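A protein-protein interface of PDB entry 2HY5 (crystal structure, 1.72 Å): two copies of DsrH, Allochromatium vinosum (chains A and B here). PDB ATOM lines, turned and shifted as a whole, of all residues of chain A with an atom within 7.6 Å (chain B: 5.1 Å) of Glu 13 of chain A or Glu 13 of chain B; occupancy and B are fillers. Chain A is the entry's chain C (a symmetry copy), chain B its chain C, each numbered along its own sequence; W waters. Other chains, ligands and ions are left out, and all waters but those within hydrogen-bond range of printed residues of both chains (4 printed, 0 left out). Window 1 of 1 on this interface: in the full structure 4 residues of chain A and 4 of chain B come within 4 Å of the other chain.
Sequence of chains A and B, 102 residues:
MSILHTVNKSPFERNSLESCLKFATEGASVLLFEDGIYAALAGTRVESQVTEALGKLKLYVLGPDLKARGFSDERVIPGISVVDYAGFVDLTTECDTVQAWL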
ATOM      1  N   LYS A   9     -21.286  13.379 -15.447  1.00  0.00           N
ATOM      2  CA  LYS A   9     -20.755  14.588 -16.067  1.00  0.00           C
ATOM      3  C   LYS A   9     -21.768  15.292 -16.954  1.00  0.00           C
ATOM      4  O   LYS A   9     -22.615  14.656 -17.577  1.00  0.00           O
ATOM      5  CB  LYS A   9     -19.507  14.240 -16.882  1.00  0.00           C
ATOM      6  CG  LYS A   9     -18.195  14.558 -16.185  1.00  0.00           C
ATOM      7  CD  LYS A   9     -18.180  14.075 -14.749  1.00  0.00           C
ATOM      8  CE  LYS A   9     -16.898  14.474 -14.034  1.00  0.00           C
ATOM      9  NZ  LYS A   9     -16.708  15.944 -13.919  1.00  0.00           N
ATOM     10  N   SER A  10     -21.663  16.615 -17.005  1.00  0.00           N
ATOM     11  CA  SER A  10     -22.546  17.438 -17.817  1.00  0.00           C
ATOM     12  C   SER A  10     -22.460  17.043 -19.288  1.00  0.00           C
ATOM     13  O   SER A  10     -21.369  16.811 -19.814  1.00  0.00           O
ATOM     14  CB  SER A  10     -22.164  18.912 -17.668  1.00  0.00           C
ATOM     15  OG  SER A  10     -22.774  19.699 -18.672  1.00  0.00           O
ATOM     16  N   PRO A  11     -23.612  16.959 -19.969  1.00  0.00           N
ATOM     17  CA  PRO A  11     -23.652  16.593 -21.385  1.00  0.00           C
ATOM     18  C   PRO A  11     -23.132  17.730 -22.262  1.00  0.00           C
ATOM     19  O   PRO A  11     -22.867  17.541 -23.446  1.00  0.00           O
ATOM     20  CB  PRO A  11     -25.131  16.299 -21.617  1.00  0.00           C
ATOM     21  CG  PRO A  11     -25.798  17.264 -20.691  1.00  0.00           C
ATOM     22  CD  PRO A  11     -24.974  17.122 -19.429  1.00  0.00           C
ATOM     23  N   PHE A  12     -22.992  18.914 -21.673  1.00  0.00           N
ATOM     24  CA  PHE A  12     -22.500  20.072 -22.410  1.00  0.00           C
ATOM     25  C   PHE A  12     -21.001  20.206 -22.190  1.00  0.00           C
ATOM     26  O   PHE A  12     -20.297  20.863 -22.960  1.00  0.00           O
ATOM     27  CB  PHE A  12     -23.203  21.340 -21.925  1.00  0.00           C
ATOM     28  CG  PHE A  12     -24.691  21.187 -21.774  1.00  0.00           C
ATOM     29  CD1 PHE A  12     -25.277  21.183 -20.513  1.00  0.00           C
ATOM     30  CD2 PHE A  12     -25.503  21.009 -22.889  1.00  0.00           C
ATOM     31  CE1 PHE A  12     -26.651  21.000 -20.364  1.00  0.00           C
ATOM     32  CE2 PHE A  12     -26.881  20.824 -22.751  1.00  0.00           C
ATOM     33  CZ  PHE A  12     -27.454  20.819 -21.486  1.00  0.00           C
ATOM     34  N   GLU A  13     -20.524  19.564 -21.131  1.00  0.00           N
ATOM     35  CA  GLU A  13     -19.118  19.603 -20.755  1.00  0.00           C
ATOM     36  C   GLU A  13     -18.326  18.399 -21.262  1.00  0.00           C
ATOM     37  O   GLU A  13     -17.229  18.555 -21.804  1.00  0.00           O
ATOM     38  CB  GLU A  13     -19.012  19.681 -19.229  1.00  0.00           C
ATOM     39  CG  GLU A  13     -17.594  19.696 -18.687  1.00  0.00           C
ATOM     40  CD  GLU A  13     -16.781  20.872 -19.196  1.00  0.00           C
ATOM     41  OE1 GLU A  13     -15.634  21.046 -18.736  1.00  0.00           O
ATOM     42  OE2 GLU A  13     -17.283  21.625 -20.060  1.00  0.00           O
ATOM     43  N   ARG A  14     -18.883  17.205 -21.079  1.00  0.00           N
ATOM     44  CA  ARG A  14     -18.223  15.963 -21.490  1.00  0.00           C
ATOM     45  C   ARG A  14     -19.042  15.130 -22.470  1.00  0.00           C
ATOM     46  O   ARG A  14     -20.250  15.330 -22.628  1.00  0.00           O
ATOM     47  CB  ARG A  14     -17.921  15.090 -20.271  1.00  0.00           C
ATOM     48  CG  ARG A  14     -16.457  15.000 -19.883  1.00  0.00           C
ATOM     49  CD  ARG A  14     -16.092  16.053 -18.859  1.00  0.00           C
ATOM     50  NE  ARG A  14     -15.028  15.586 -17.975  1.00  0.00           N
ATOM     51  CZ  ARG A  14     -14.563  16.276 -16.939  1.00  0.00           C
ATOM     52  NH1 ARG A  14     -15.068  17.468 -16.656  1.00  0.00           N
ATOM     53  NH2 ARG A  14     -13.602  15.768 -16.180  1.00  0.00           N
ATOM     54  N   ASN A  15     -18.369  14.167 -23.094  1.00  0.00           N
ATOM     55  CA  ASN A  15     -18.978  13.274 -24.073  1.00  0.00           C
ATOM     56  C   ASN A  15     -19.522  11.997 -23.428  1.00  0.00           C
ATOM     57  O   ASN A  15     -20.001  11.104 -24.120  1.00  0.00           O
ATOM     58  CB  ASN A  15     -17.935  12.899 -25.125  1.00  0.00           C
ATOM     59  CG  ASN A  15     -16.845  11.995 -24.573  1.00  0.00           C
ATOM     60  OD1 ASN A  15     -16.418  12.140 -23.426  1.00  0.00           O
ATOM     61  ND2 ASN A  15     -16.382  11.058 -25.396  1.00  0.00           N
ATOM     62  N   SER A  16     -19.457  11.927 -22.105  1.00  0.00           N
ATOM     63  CA  SER A  16     -19.900  10.751 -21.361  1.00  0.00           C
ATOM     64  C   SER A  16     -21.334  10.307 -21.627  1.00  0.00           C
ATOM     65  O   SER A  16     -21.583   9.127 -21.879  1.00  0.00           O
ATOM     66  CB  SER A  16     -19.715  10.989 -19.864  1.00  0.00           C
ATOM     67  OG  SER A  16     -18.353  11.225 -19.569  1.00  0.00           O
ATOM     68  N   SER A  19     -21.820   8.903 -25.251  1.00  0.00           N
ATOM     69  CA  SER A  19     -21.256   7.571 -25.427  1.00  0.00           C
ATOM     70  C   SER A  19     -22.149   6.531 -24.752  1.00  0.00           C
ATOM     71  O   SER A  19     -22.369   5.443 -25.280  1.00  0.00           O
ATOM     72  CB  SER A  19     -19.850   7.501 -24.830  1.00  0.00           C
ATOM     73  OG  SER A  19     -18.995   8.445 -25.451  1.00  0.00           O
ATOM     74  N   ASP A  35     -23.200  16.272 -11.888  1.00  0.00           N
ATOM     75  CA  ASP A  35     -23.413  17.171 -13.019  1.00  0.00           C
ATOM     76  C   ASP A  35     -24.168  16.531 -14.191  1.00  0.00           C
ATOM     77  O   ASP A  35     -24.592  17.227 -15.121  1.00  0.00           O
ATOM     78  CB  ASP A  35     -22.069  17.728 -13.501  1.00  0.00           C
ATOM     79  CG  ASP A  35     -21.469  18.737 -12.531  1.00  0.00           C
ATOM     80  OD1 ASP A  35     -20.309  19.149 -12.752  1.00  0.00           O
ATOM     81  OD2 ASP A  35     -22.150  19.139 -11.555  1.00  0.00           O
ATOM     82  N   ARG A  45     -30.281  21.727 -25.225  1.00  0.00           N
ATOM     83  CA  ARG A  45     -29.881  21.340 -26.572  1.00  0.00           C
ATOM     84  C   ARG A  45     -29.788  19.821 -26.744  1.00  0.00           C
ATOM     85  O   ARG A  45     -29.673  19.328 -27.866  1.00  0.00           O
ATOM     86  CB  ARG A  45     -28.533  21.980 -26.917  1.00  0.00           C
ATOM     87  CG  ARG A  45     -28.210  21.983 -28.400  1.00  0.00           C
ATOM     88  CD  ARG A  45     -26.795  22.474 -28.665  1.00  0.00           C
ATOM     89  NE  ARG A  45     -25.797  21.594 -28.064  1.00  0.00           N
ATOM     90  CZ  ARG A  45     -25.116  21.875 -26.957  1.00  0.00           C
ATOM     91  NH1 ARG A  45     -25.321  23.020 -26.323  1.00  0.00           N
ATOM     92  NH2 ARG A  45     -24.233  21.009 -26.481  1.00  0.00           N
ATOM     93  N   LEU A 102     -17.405   7.848 -16.624  1.00  0.00           N
ATOM     94  CA  LEU A 102     -16.763   9.001 -15.999  1.00  0.00           C
ATOM     95  C   LEU A 102     -16.465  10.127 -16.987  1.00  0.00           C
ATOM     96  O   LEU A 102     -15.290  10.249 -17.388  1.00  0.00           O
ATOM     97  CB  LEU A 102     -15.477   8.545 -15.293  1.00  0.00           C
ATOM     98  CG  LEU A 102     -15.728   7.419 -14.273  1.00  0.00           C
ATOM     99  CD1 LEU A 102     -14.421   7.007 -13.617  1.00  0.00           C
ATOM    100  CD2 LEU A 102     -16.722   7.873 -13.209  1.00  0.00           C
ATOM    101  OXT LEU A 102     -17.400  10.873 -17.350  1.00  0.00           O
ATOM    102  N   SER B  10      -8.867  17.342 -24.749  1.00  0.00           N
ATOM    103  CA  SER B  10      -9.242  16.699 -25.999  1.00  0.00           C
ATOM    104  C   SER B  10     -10.552  17.269 -26.534  1.00  0.00           C
ATOM    105  O   SER B  10     -11.501  17.481 -25.776  1.00  0.00           O
ATOM    106  CB  SER B  10      -9.400  15.193 -25.780  1.00  0.00           C
ATOM    107  OG  SER B  10     -10.067  14.589 -26.871  1.00  0.00           O
ATOM    108  N   PRO B  11     -10.617  17.528 -27.848  1.00  0.00           N
ATOM    109  CA  PRO B  11     -11.823  18.072 -28.473  1.00  0.00           C
ATOM    110  C   PRO B  11     -12.926  17.018 -28.552  1.00  0.00           C
ATOM    111  O   PRO B  11     -14.080  17.334 -28.825  1.00  0.00           O
ATOM    112  CB  PRO B  11     -11.325  18.506 -29.849  1.00  0.00           C
ATOM    113  CG  PRO B  11     -10.273  17.486 -30.144  1.00  0.00           C
ATOM    114  CD  PRO B  11      -9.525  17.403 -28.831  1.00  0.00           C
ATOM    115  N   PHE B  12     -12.561  15.762 -28.313  1.00  0.00           N
ATOM    116  CA  PHE B  12     -13.528  14.672 -28.356  1.00  0.00           C
ATOM    117  C   PHE B  12     -14.034  14.396 -26.948  1.00  0.00           C
ATOM    118  O   PHE B  12     -15.090  13.789 -26.754  1.00  0.00           O
ATOM    119  CB  PHE B  12     -12.873  13.410 -28.920  1.00  0.00           C
ATOM    120  CG  PHE B  12     -12.043  13.658 -30.148  1.00  0.00           C
ATOM    121  CD1 PHE B  12     -10.658  13.548 -30.099  1.00  0.00           C
ATOM    122  CD2 PHE B  12     -12.642  14.037 -31.345  1.00  0.00           C
ATOM    123  CE1 PHE B  12      -9.879  13.816 -31.224  1.00  0.00           C
ATOM    124  CE2 PHE B  12     -11.870  14.309 -32.478  1.00  0.00           C
ATOM    125  CZ  PHE B  12     -10.488  14.198 -32.416  1.00  0.00           C
ATOM    126  N   GLU B  13     -13.267  14.860 -25.969  1.00  0.00           N
ATOM    127  CA  GLU B  13     -13.585  14.666 -24.561  1.00  0.00           C
ATOM    128  C   GLU B  13     -14.306  15.859 -23.937  1.00  0.00           C
ATOM    129  O   GLU B  13     -15.302  15.689 -23.229  1.00  0.00           O
ATOM    130  CB  GLU B  13     -12.290  14.387 -23.792  1.00  0.00           C
ATOM    131  CG  GLU B  13     -12.465  14.194 -22.296  1.00  0.00           C
ATOM    132  CD  GLU B  13     -13.380  13.033 -21.954  1.00  0.00           C
ATOM    133  OE1 GLU B  13     -13.516  12.715 -20.755  1.00  0.00           O
ATOM    134  OE2 GLU B  13     -13.971  12.437 -22.881  1.00  0.00           O
ATOM    135  N   ARG B  14     -13.795  17.060 -24.196  1.00  0.00           N
ATOM    136  CA  ARG B  14     -14.367  18.289 -23.640  1.00  0.00           C
ATOM    137  C   ARG B  14     -14.792  19.301 -24.700  1.00  0.00           C
ATOM    138  O   ARG B  14     -14.391  19.215 -25.864  1.00  0.00           O
ATOM    139  CB  ARG B  14     -13.360  18.975 -22.715  1.00  0.00           C
ATOM    140  CG  ARG B  14     -13.684  18.902 -21.235  1.00  0.00           C
ATOM    141  CD  ARG B  14     -13.028  17.703 -20.585  1.00  0.00           C
ATOM    142  NE  ARG B  14     -12.700  17.971 -19.187  1.00  0.00           N
ATOM    143  CZ  ARG B  14     -12.051  17.122 -18.398  1.00  0.00           C
ATOM    144  NH1 ARG B  14     -11.660  15.947 -18.868  1.00  0.00           N
ATOM    145  NH2 ARG B  14     -11.783  17.454 -17.143  1.00  0.00           N
ATOM    146  N   ASN B  15     -15.579  20.279 -24.263  1.00  0.00           N
ATOM    147  CA  ASN B  15     -16.096  21.333 -25.128  1.00  0.00           C
ATOM    148  C   ASN B  15     -15.176  22.557 -25.159  1.00  0.00           C
ATOM    149  O   ASN B  15     -15.499  23.564 -25.779  1.00  0.00           O
ATOM    150  CB  ASN B  15     -17.478  21.757 -24.631  1.00  0.00           C
ATOM    151  CG  ASN B  15     -17.421  22.497 -23.305  1.00  0.00           C
ATOM    152  OD1 ASN B  15     -16.615  22.175 -22.430  1.00  0.00           O
ATOM    153  ND2 ASN B  15     -18.290  23.492 -23.147  1.00  0.00           N
ATOM    154  N   LEU B 102      -9.814  25.636 -19.704  1.00  0.00           N
ATOM    155  CA  LEU B 102      -9.646  24.368 -19.001  1.00  0.00           C
ATOM    156  C   LEU B 102     -10.744  23.356 -19.324  1.00  0.00           C
ATOM    157  O   LEU B 102     -11.649  23.195 -18.480  1.00  0.00           O
ATOM    158  CB  LEU B 102      -9.578  24.630 -17.489  1.00  0.00           C
ATOM    159  CG  LEU B 102      -8.474  25.634 -17.111  1.00  0.00           C
ATOM    160  CD1 LEU B 102      -8.464  25.858 -15.608  1.00  0.00           C
ATOM    161  CD2 LEU B 102      -7.111  25.127 -17.568  1.00  0.00           C
ATOM    162  OXT LEU B 102     -10.692  22.736 -20.408  1.00  0.00           O
HETATM  163  O   HOH W   1     -19.480  23.439 -20.137  1.00  0.00           O
HETATM  164  O   HOH W   2     -14.818  23.520 -18.687  1.00  0.00           O
HETATM  165  O   HOH W   3     -13.168  10.821 -25.089  1.00  0.00           O
HETATM  166  O   HOH W   4     -14.038  10.199 -20.324  1.00  0.00           O
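Glu 13 of chain A touches Glu 13 of chain B. O of Glu 13 of chain A touches CA of Arg 14 of chain B, 3.4 Å away. Arg 14 of chain A touches Glu 13 of chain B.
Water W2 bridges the side-chain carboxylate (OE1) of Glu 13 of chain A and the chain-end carboxylate (O) of Leu 102 of chain B. Water W4 lies within hydrogen-bond range of OE1 of Glu 13 of chain B (2.6 Å) and O of Leu 102 of chain A (3.2 Å). Water W3 bridges the side-chain carboxylate (OE2) of Glu 13 of chain B and the side-chain amide nitrogen (ND2) of Asn 15 of chain A. Water W1 bridges the side-chain carboxylate of Glu 13 of chain A (2.9 Å) and the side-chain amide nitrogen of Asn 15 of chain B (3.2 Å).
Phe 12 of chain A touches Asn 15 of chain B, and with the chains exchanged Asn 15 of chain A touches Phe 12 of chain B. Glu 13 of chain A touches its own counterpart, Glu 13 of chain B. Glu 13 of chain A touches Arg 14 of chain B, and with the chains exchanged Arg 14 of chain A touches Glu 13 of chain B. Arg 14 of chain A touches its own counterpart, Arg 14 of chain B. Positions printed for both chains: 10, 11, 12, 13, 14, 15 and 102.
Glu 13 of chain A touches just these residues of chain B: Glu 13, Arg 14 and Asn 15. Of chain A, only Glu 13, Arg 14 and Asn 15 come within 4 Å of Glu 13 of chain B. Of the printed residues of chain B, Phe 12 of chain A touches Asn 15 (3.3 Å). Printed residues of chain B within 4 Å of Asn 15 of chain A: Phe 12 and Glu 13. Pro 11 of chain B touches none of the printed residues of chain A. The nearest residue of chain B that does not touch Glu 13 of chain A is Leu 102 of chain B (4.5 Å). The nearest printed residue of chain B that does not touch Phe 12 of chain A is Arg 14 of chain B (6.0 Å).
The backbone NH of Phe 12 of chain B lies close to the side-chain hydroxyl of Ser 10 of chain B (3.1 Å). The side-chain hydroxyl of Ser 10 of chain B lies within hydrogen-bond range of the backbone NH of Glu 13 of chain B, at 3.3 Å. The side-chain hydroxyl (OG) of Ser 10 of chain A sits close to the backbone NH (N) of Phe 12 of chain A, 3.1 Å away. The side-chain hydroxyl (OG) of Ser 10 of chain A lies within hydrogen-bond range of the backbone NH (N) of Glu 13 of chain A, at 3.3 Å. The backbone carbonyl oxygen of Asn 15 of chain A is in hydrogen-bond range of the side-chain hydroxyl of Ser 19 of chain A.
O of Phe 12 of chain B lies within hydrogen-bond range of ND2 of Asn 15 of chain A (3.3 Å). The side-chain carboxylate of Glu 13 of chain B lies close to the side-chain amide oxygen of Asn 15 of chain A (2.5 Å). NH2 of Arg 14 of chain A lies close to NH2 of Arg 14 of chain B, 2.7 Å away. ND2 of Asn 15 of chain B sits at hydrogen-bond distance from O of Phe 12 of chain A, at 3.3 Å. OD1 of Asn 15 of chain B lies close to OE2 of Glu 13 of chain A.
Of the 7 printed residues of chain B, 4 touch a printed residue of chain A. Among the printed residues, no Asp or Glu carboxylate lies within 4 Å of a Lys or Arg side-chain nitrogen of the other chain.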
